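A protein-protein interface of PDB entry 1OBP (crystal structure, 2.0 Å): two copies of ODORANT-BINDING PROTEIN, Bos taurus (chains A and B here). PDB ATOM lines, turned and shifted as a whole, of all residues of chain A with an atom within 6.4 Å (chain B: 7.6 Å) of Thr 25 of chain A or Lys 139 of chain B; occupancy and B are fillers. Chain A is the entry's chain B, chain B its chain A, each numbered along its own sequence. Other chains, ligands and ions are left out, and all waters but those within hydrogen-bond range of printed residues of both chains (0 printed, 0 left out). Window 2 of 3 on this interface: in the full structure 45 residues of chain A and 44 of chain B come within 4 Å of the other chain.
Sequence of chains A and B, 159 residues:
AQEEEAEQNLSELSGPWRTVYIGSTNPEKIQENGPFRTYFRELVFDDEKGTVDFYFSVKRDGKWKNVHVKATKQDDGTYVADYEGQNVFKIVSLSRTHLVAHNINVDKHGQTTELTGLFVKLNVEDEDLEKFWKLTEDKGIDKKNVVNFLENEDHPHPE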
ATOM      1  N   GLY A  23     -23.382   6.616  -3.944  1.00  0.00           N
ATOM      2  CA  GLY A  23     -24.781   6.348  -3.596  1.00  0.00           C
ATOM      3  C   GLY A  23     -24.839   5.178  -2.600  1.00  0.00           C
ATOM      4  O   GLY A  23     -23.920   4.354  -2.616  1.00  0.00           O
ATOM      5  N   SER A  24     -25.893   5.058  -1.779  1.00  0.00           N
ATOM      6  CA  SER A  24     -25.982   3.958  -0.799  1.00  0.00           C
ATOM      7  C   SER A  24     -27.400   3.453  -0.558  1.00  0.00           C
ATOM      8  O   SER A  24     -28.327   4.269  -0.466  1.00  0.00           O
ATOM      9  CB  SER A  24     -25.449   4.440   0.557  1.00  0.00           C
ATOM     10  OG  SER A  24     -25.658   3.478   1.591  1.00  0.00           O
ATOM     11  N   THR A  25     -27.560   2.139  -0.370  1.00  0.00           N
ATOM     12  CA  THR A  25     -28.887   1.578  -0.077  1.00  0.00           C
ATOM     13  C   THR A  25     -29.269   1.967   1.358  1.00  0.00           C
ATOM     14  O   THR A  25     -30.450   1.954   1.724  1.00  0.00           O
ATOM     15  CB  THR A  25     -28.949   0.039  -0.198  1.00  0.00           C
ATOM     16  OG1 THR A  25     -27.915  -0.552   0.592  1.00  0.00           O
ATOM     17  CG2 THR A  25     -28.786  -0.391  -1.624  1.00  0.00           C
ATOM     18  N   ASN A  26     -28.275   2.324   2.170  1.00  0.00           N
ATOM     19  CA  ASN A  26     -28.517   2.744   3.557  1.00  0.00           C
ATOM     20  C   ASN A  26     -27.963   4.170   3.659  1.00  0.00           C
ATOM     21  O   ASN A  26     -26.740   4.394   3.717  1.00  0.00           O
ATOM     22  CB  ASN A  26     -27.812   1.792   4.549  1.00  0.00           C
ATOM     23  CG  ASN A  26     -28.135   2.097   6.000  1.00  0.00           C
ATOM     24  OD1 ASN A  26     -28.702   3.145   6.327  1.00  0.00           O
ATOM     25  ND2 ASN A  26     -27.745   1.192   6.892  1.00  0.00           N
ATOM     26  N   PRO A  27     -28.860   5.161   3.633  1.00  0.00           N
ATOM     27  CA  PRO A  27     -28.466   6.568   3.716  1.00  0.00           C
ATOM     28  C   PRO A  27     -27.611   6.927   4.925  1.00  0.00           C
ATOM     29  O   PRO A  27     -26.725   7.768   4.822  1.00  0.00           O
ATOM     30  CB  PRO A  27     -29.810   7.310   3.717  1.00  0.00           C
ATOM     31  CG  PRO A  27     -30.820   6.267   4.196  1.00  0.00           C
ATOM     32  CD  PRO A  27     -30.325   5.016   3.522  1.00  0.00           C
ATOM     33  N   HIS A 102     -18.814  -0.817  -7.577  1.00  0.00           N
ATOM     34  CA  HIS A 102     -19.929  -1.304  -6.761  1.00  0.00           C
ATOM     35  C   HIS A 102     -19.279  -1.972  -5.526  1.00  0.00           C
ATOM     36  O   HIS A 102     -18.441  -2.849  -5.679  1.00  0.00           O
ATOM     37  CB  HIS A 102     -20.749  -2.329  -7.576  1.00  0.00           C
ATOM     38  CG  HIS A 102     -21.796  -3.047  -6.779  1.00  0.00           C
ATOM     39  ND1 HIS A 102     -22.073  -4.387  -6.956  1.00  0.00           N
ATOM     40  CD2 HIS A 102     -22.588  -2.632  -5.761  1.00  0.00           C
ATOM     41  CE1 HIS A 102     -22.982  -4.770  -6.076  1.00  0.00           C
ATOM     42  NE2 HIS A 102     -23.311  -3.726  -5.335  1.00  0.00           N
ATOM     43  N   THR A 112     -26.092  -5.489   5.893  1.00  0.00           N
ATOM     44  CA  THR A 112     -25.532  -5.314   4.540  1.00  0.00           C
ATOM     45  C   THR A 112     -25.965  -4.009   3.841  1.00  0.00           C
ATOM     46  O   THR A 112     -27.131  -3.582   3.922  1.00  0.00           O
ATOM     47  CB  THR A 112     -25.842  -6.551   3.645  1.00  0.00           C
ATOM     48  OG1 THR A 112     -25.405  -6.320   2.297  1.00  0.00           O
ATOM     49  CG2 THR A 112     -27.324  -6.840   3.622  1.00  0.00           C
ATOM     50  N   THR A 113     -25.000  -3.365   3.197  1.00  0.00           N
ATOM     51  CA  THR A 113     -25.205  -2.099   2.480  1.00  0.00           C
ATOM     52  C   THR A 113     -24.487  -2.224   1.155  1.00  0.00           C
ATOM     53  O   THR A 113     -23.388  -2.773   1.099  1.00  0.00           O
ATOM     54  CB  THR A 113     -24.552  -0.886   3.215  1.00  0.00           C
ATOM     55  OG1 THR A 113     -24.979  -0.833   4.585  1.00  0.00           O
ATOM     56  CG2 THR A 113     -24.939   0.436   2.548  1.00  0.00           C
ATOM     57  N   GLU A 114     -25.144  -1.811   0.075  1.00  0.00           N
ATOM     58  CA  GLU A 114     -24.515  -1.842  -1.245  1.00  0.00           C
ATOM     59  C   GLU A 114     -24.314  -0.380  -1.648  1.00  0.00           C
ATOM     60  O   GLU A 114     -25.166   0.475  -1.380  1.00  0.00           O
ATOM     61  CB  GLU A 114     -25.365  -2.614  -2.242  1.00  0.00           C
ATOM     62  CG  GLU A 114     -25.735  -4.011  -1.699  1.00  0.00           C
ATOM     63  CD  GLU A 114     -25.880  -5.045  -2.772  1.00  0.00           C
ATOM     64  OE1 GLU A 114     -25.479  -4.811  -3.922  1.00  0.00           O
ATOM     65  OE2 GLU A 114     -26.365  -6.137  -2.459  1.00  0.00           O
ATOM     66  N   LEU A 115     -23.131  -0.088  -2.178  1.00  0.00           N
ATOM     67  CA  LEU A 115     -22.759   1.266  -2.543  1.00  0.00           C
ATOM     68  C   LEU A 115     -22.240   1.341  -3.956  1.00  0.00           C
ATOM     69  O   LEU A 115     -21.744   0.353  -4.486  1.00  0.00           O
ATOM     70  CB  LEU A 115     -21.689   1.785  -1.561  1.00  0.00           C
ATOM     71  CG  LEU A 115     -22.123   1.904  -0.086  1.00  0.00           C
ATOM     72  CD1 LEU A 115     -21.528   0.763   0.755  1.00  0.00           C
ATOM     73  CD2 LEU A 115     -21.687   3.243   0.498  1.00  0.00           C
ATOM     74  N   THR A 116     -22.439   2.495  -4.595  1.00  0.00           N
ATOM     75  CA  THR A 116     -21.957   2.720  -5.957  1.00  0.00           C
ATOM     76  C   THR A 116     -21.175   4.041  -5.889  1.00  0.00           C
ATOM     77  O   THR A 116     -21.519   4.912  -5.080  1.00  0.00           O
ATOM     78  CB  THR A 116     -23.127   2.849  -6.970  1.00  0.00           C
ATOM     79  OG1 THR A 116     -23.989   3.909  -6.552  1.00  0.00           O
ATOM     80  CG2 THR A 116     -23.939   1.538  -7.023  1.00  0.00           C
ATOM     81  N   TRP B 133     -25.095   6.047 -13.281  1.00  0.00           N
ATOM     82  CA  TRP B 133     -26.541   6.135 -13.014  1.00  0.00           C
ATOM     83  C   TRP B 133     -27.270   4.832 -13.322  1.00  0.00           C
ATOM     84  O   TRP B 133     -28.182   4.473 -12.587  1.00  0.00           O
ATOM     85  CB  TRP B 133     -27.204   7.316 -13.734  1.00  0.00           C
ATOM     86  CG  TRP B 133     -26.844   8.625 -13.139  1.00  0.00           C
ATOM     87  CD1 TRP B 133     -26.085   9.609 -13.717  1.00  0.00           C
ATOM     88  CD2 TRP B 133     -27.185   9.099 -11.831  1.00  0.00           C
ATOM     89  NE1 TRP B 133     -25.931  10.658 -12.847  1.00  0.00           N
ATOM     90  CE2 TRP B 133     -26.595  10.375 -11.683  1.00  0.00           C
ATOM     91  CE3 TRP B 133     -27.920   8.568 -10.766  1.00  0.00           C
ATOM     92  CZ2 TRP B 133     -26.718  11.128 -10.518  1.00  0.00           C
ATOM     93  CZ3 TRP B 133     -28.039   9.322  -9.600  1.00  0.00           C
ATOM     94  CH2 TRP B 133     -27.443  10.582  -9.489  1.00  0.00           C
ATOM     95  N   LYS B 134     -26.868   4.116 -14.370  1.00  0.00           N
ATOM     96  CA  LYS B 134     -27.502   2.836 -14.690  1.00  0.00           C
ATOM     97  C   LYS B 134     -27.200   1.850 -13.547  1.00  0.00           C
ATOM     98  O   LYS B 134     -28.103   1.223 -12.991  1.00  0.00           O
ATOM     99  CB  LYS B 134     -26.957   2.271 -15.992  1.00  0.00           C
ATOM    100  CG  LYS B 134     -27.610   0.933 -16.422  1.00  0.00           C
ATOM    101  CD  LYS B 134     -26.550  -0.071 -16.892  1.00  0.00           C
ATOM    102  CE  LYS B 134     -27.135  -1.290 -17.612  1.00  0.00           C
ATOM    103  NZ  LYS B 134     -27.858  -2.224 -16.716  1.00  0.00           N
ATOM    104  N   LEU B 135     -25.927   1.761 -13.162  1.00  0.00           N
ATOM    105  CA  LEU B 135     -25.511   0.879 -12.067  1.00  0.00           C
ATOM    106  C   LEU B 135     -26.263   1.214 -10.796  1.00  0.00           C
ATOM    107  O   LEU B 135     -26.745   0.323 -10.098  1.00  0.00           O
ATOM    108  CB  LEU B 135     -23.999   0.987 -11.801  1.00  0.00           C
ATOM    109  CG  LEU B 135     -23.460   0.158 -10.627  1.00  0.00           C
ATOM    110  CD1 LEU B 135     -23.474  -1.327 -10.998  1.00  0.00           C
ATOM    111  CD2 LEU B 135     -22.029   0.601 -10.263  1.00  0.00           C
ATOM    112  N   THR B 136     -26.395   2.505 -10.521  1.00  0.00           N
ATOM    113  CA  THR B 136     -27.079   2.965  -9.318  1.00  0.00           C
ATOM    114  C   THR B 136     -28.552   2.517  -9.298  1.00  0.00           C
ATOM    115  O   THR B 136     -29.103   2.145  -8.250  1.00  0.00           O
ATOM    116  CB  THR B 136     -26.937   4.502  -9.194  1.00  0.00           C
ATOM    117  OG1 THR B 136     -25.557   4.816  -8.992  1.00  0.00           O
ATOM    118  CG2 THR B 136     -27.722   5.051  -8.054  1.00  0.00           C
ATOM    119  N   GLU B 137     -29.166   2.549 -10.473  1.00  0.00           N
ATOM    120  CA  GLU B 137     -30.555   2.160 -10.669  1.00  0.00           C
ATOM    121  C   GLU B 137     -30.645   0.634 -10.509  1.00  0.00           C
ATOM    122  O   GLU B 137     -31.560   0.121  -9.859  1.00  0.00           O
ATOM    123  CB  GLU B 137     -30.974   2.582 -12.075  1.00  0.00           C
ATOM    124  CG  GLU B 137     -32.454   2.576 -12.348  1.00  0.00           C
ATOM    125  CD  GLU B 137     -32.797   3.185 -13.714  1.00  0.00           C
ATOM    126  OE1 GLU B 137     -31.868   3.492 -14.507  1.00  0.00           O
ATOM    127  OE2 GLU B 137     -34.007   3.359 -13.996  1.00  0.00           O
ATOM    128  N   ASP B 138     -29.679  -0.082 -11.084  1.00  0.00           N
ATOM    129  CA  ASP B 138     -29.636  -1.540 -10.993  1.00  0.00           C
ATOM    130  C   ASP B 138     -29.665  -2.036  -9.543  1.00  0.00           C
ATOM    131  O   ASP B 138     -30.290  -3.056  -9.253  1.00  0.00           O
ATOM    132  CB  ASP B 138     -28.383  -2.100 -11.669  1.00  0.00           C
ATOM    133  CG  ASP B 138     -28.435  -2.030 -13.181  1.00  0.00           C
ATOM    134  OD1 ASP B 138     -29.488  -1.665 -13.746  1.00  0.00           O
ATOM    135  OD2 ASP B 138     -27.399  -2.338 -13.808  1.00  0.00           O
ATOM    136  N   LYS B 139     -28.971  -1.329  -8.646  1.00  0.00           N
ATOM    137  CA  LYS B 139     -28.890  -1.704  -7.221  1.00  0.00           C
ATOM    138  C   LYS B 139     -30.019  -1.123  -6.401  1.00  0.00           C
ATOM    139  O   LYS B 139     -29.984  -1.175  -5.171  1.00  0.00           O
ATOM    140  CB  LYS B 139     -27.546  -1.276  -6.598  1.00  0.00           C
ATOM    141  CG  LYS B 139     -26.283  -1.662  -7.392  1.00  0.00           C
ATOM    142  CD  LYS B 139     -25.972  -3.164  -7.376  1.00  0.00           C
ATOM    143  CE  LYS B 139     -26.303  -3.855  -8.663  1.00  0.00           C
ATOM    144  NZ  LYS B 139     -26.082  -5.315  -8.531  1.00  0.00           N
ATOM    145  N   GLY B 140     -31.008  -0.549  -7.081  1.00  0.00           N
ATOM    146  CA  GLY B 140     -32.171   0.019  -6.418  1.00  0.00           C
ATOM    147  C   GLY B 140     -31.902   1.185  -5.493  1.00  0.00           C
ATOM    148  O   GLY B 140     -32.598   1.358  -4.468  1.00  0.00           O
ATOM    149  N   ILE B 141     -30.913   2.010  -5.822  1.00  0.00           N
ATOM    150  CA  ILE B 141     -30.624   3.146  -4.952  1.00  0.00           C
ATOM    151  C   ILE B 141     -31.395   4.367  -5.431  1.00  0.00           C
ATOM    152  O   ILE B 141     -31.400   4.678  -6.621  1.00  0.00           O
ATOM    153  CB  ILE B 141     -29.093   3.463  -4.884  1.00  0.00           C
ATOM    154  CG1 ILE B 141     -28.346   2.340  -4.139  1.00  0.00           C
ATOM    155  CG2 ILE B 141     -28.870   4.794  -4.154  1.00  0.00           C
ATOM    156  CD1 ILE B 141     -26.905   2.176  -4.560  1.00  0.00           C
ATOM    157  N   ASP B 142     -32.045   5.044  -4.496  1.00  0.00           N
ATOM    158  CA  ASP B 142     -32.829   6.245  -4.780  1.00  0.00           C
ATOM    159  C   ASP B 142     -31.881   7.452  -5.009  1.00  0.00           C
ATOM    160  O   ASP B 142     -30.902   7.606  -4.286  1.00  0.00           O
ATOM    161  CB  ASP B 142     -33.756   6.480  -3.567  1.00  0.00           C
ATOM    162  CG  ASP B 142     -34.704   7.675  -3.729  1.00  0.00           C
ATOM    163  OD1 ASP B 142     -35.135   8.000  -4.862  1.00  0.00           O
ATOM    164  OD2 ASP B 142     -35.049   8.272  -2.683  1.00  0.00           O
ATOM    165  N   ASN B 145     -30.532   9.342  -2.291  1.00  0.00           N
ATOM    166  CA  ASN B 145     -29.474   8.715  -1.519  1.00  0.00           C
ATOM    167  C   ASN B 145     -28.088   8.783  -2.177  1.00  0.00           C
ATOM    168  O   ASN B 145     -27.265   7.887  -1.977  1.00  0.00           O
ATOM    169  CB  ASN B 145     -29.847   7.259  -1.182  1.00  0.00           C
ATOM    170  CG  ASN B 145     -31.030   7.160  -0.222  1.00  0.00           C
ATOM    171  OD1 ASN B 145     -31.300   8.088   0.544  1.00  0.00           O
ATOM    172  ND2 ASN B 145     -31.726   6.029  -0.247  1.00  0.00           N
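Printed residues of chain A that touch a printed residue of chain B: Gly 23, Ser 24, Thr 25, Pro 27, His 102, Glu 114 and Thr 116. Of the 11 printed residues of chain B, 5 touch a printed residue of chain A. Among the printed residues, 12 pairs touch across the chains. Among the printed residues, no Asp or Glu carboxylate lies within 4 Å of a Lys or Arg side-chain nitrogen of the other chain.
O of Thr 136 of chain B lies within hydrogen-bond range of N of Ile 141 of chain B (3.0 Å). The backbone NH (N) of Gly 23 of chain A sits at hydrogen-bond distance from the backbone carbonyl oxygen (O) of Thr 116 of chain A (2.8 Å). The side-chain hydroxyl of Ser 24 of chain A sits at hydrogen-bond distance from the backbone carbonyl oxygen of Asn 26 of chain A, 2.6 Å away. N of Thr 25 of chain A lies within hydrogen-bond range of O of Glu 114 of chain A. OE1 of Glu 114 of chain A is in hydrogen-bond range of NE2 of His 102 of chain A.
Asn 145 of chain B touches Gly 23 of chain A. Ser 24 of chain A touches Ile 141 of chain B. O of Lys 139 of chain B touches CG2 of Thr 25 of chain A (3.8 Å). Ile 141 of chain B touches Thr 25 of chain A. Pro 27 of chain A touches Asn 145 of chain B. Lys 139 of chain B touches His 102 of chain A (CD to NE2, 3.4 Å). Lys 139 of chain B touches Glu 114 of chain A. CD2 of Leu 135 of chain B touches CG2 of Thr 116 of chain A (3.9 Å). CG of Lys 139 of chain B touches CG2 of Thr 116 of chain A (3.98 Å). Thr 116 of chain A touches Ile 141 of chain B (CG2 to CD1, 3.9 Å).
No position is printed for both chains. Of the 12 pairs that touch across the chains among the printed residues, none has its exchanged pair printed and touching as well.
The side-chain hydroxyl of Thr 136 of chain B is in hydrogen-bond range of the side-chain hydroxyl of Thr 116 of chain A. The backbone NH of Ser 24 of chain A is in hydrogen-bond range of the backbone carbonyl oxygen of Asn 145 of chain B (3.2 Å).
Of chain B, only Lys 139 (3.8 Å) and Ile 141 (3.7 Å) come within 4 Å of Thr 25 of chain A. Of the printed residues of chain A, Lys 139 of chain B touches Thr 25 (3.8 Å), His 102 (3.4 Å), Glu 114 (3.9 Å) and Thr 116 (3.98 Å). Printed residues of chain A within 4 Å of Leu 135 of chain B: Thr 116 (3.9 Å). Of the printed residues of chain B, Pro 27 of chain A touches Asn 145 (3.6 Å). Of the printed residues of chain B, His 102 of chain A touches Lys 139. Printed residues of chain B within 4 Å of Ser 24 of chain A: Ile 141 (3.8 Å) and Asn 145 (3.2 Å). The nearest printed residue of chain B that does not touch His 102 of chain A is Leu 135 of chain B (4.2 Å).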
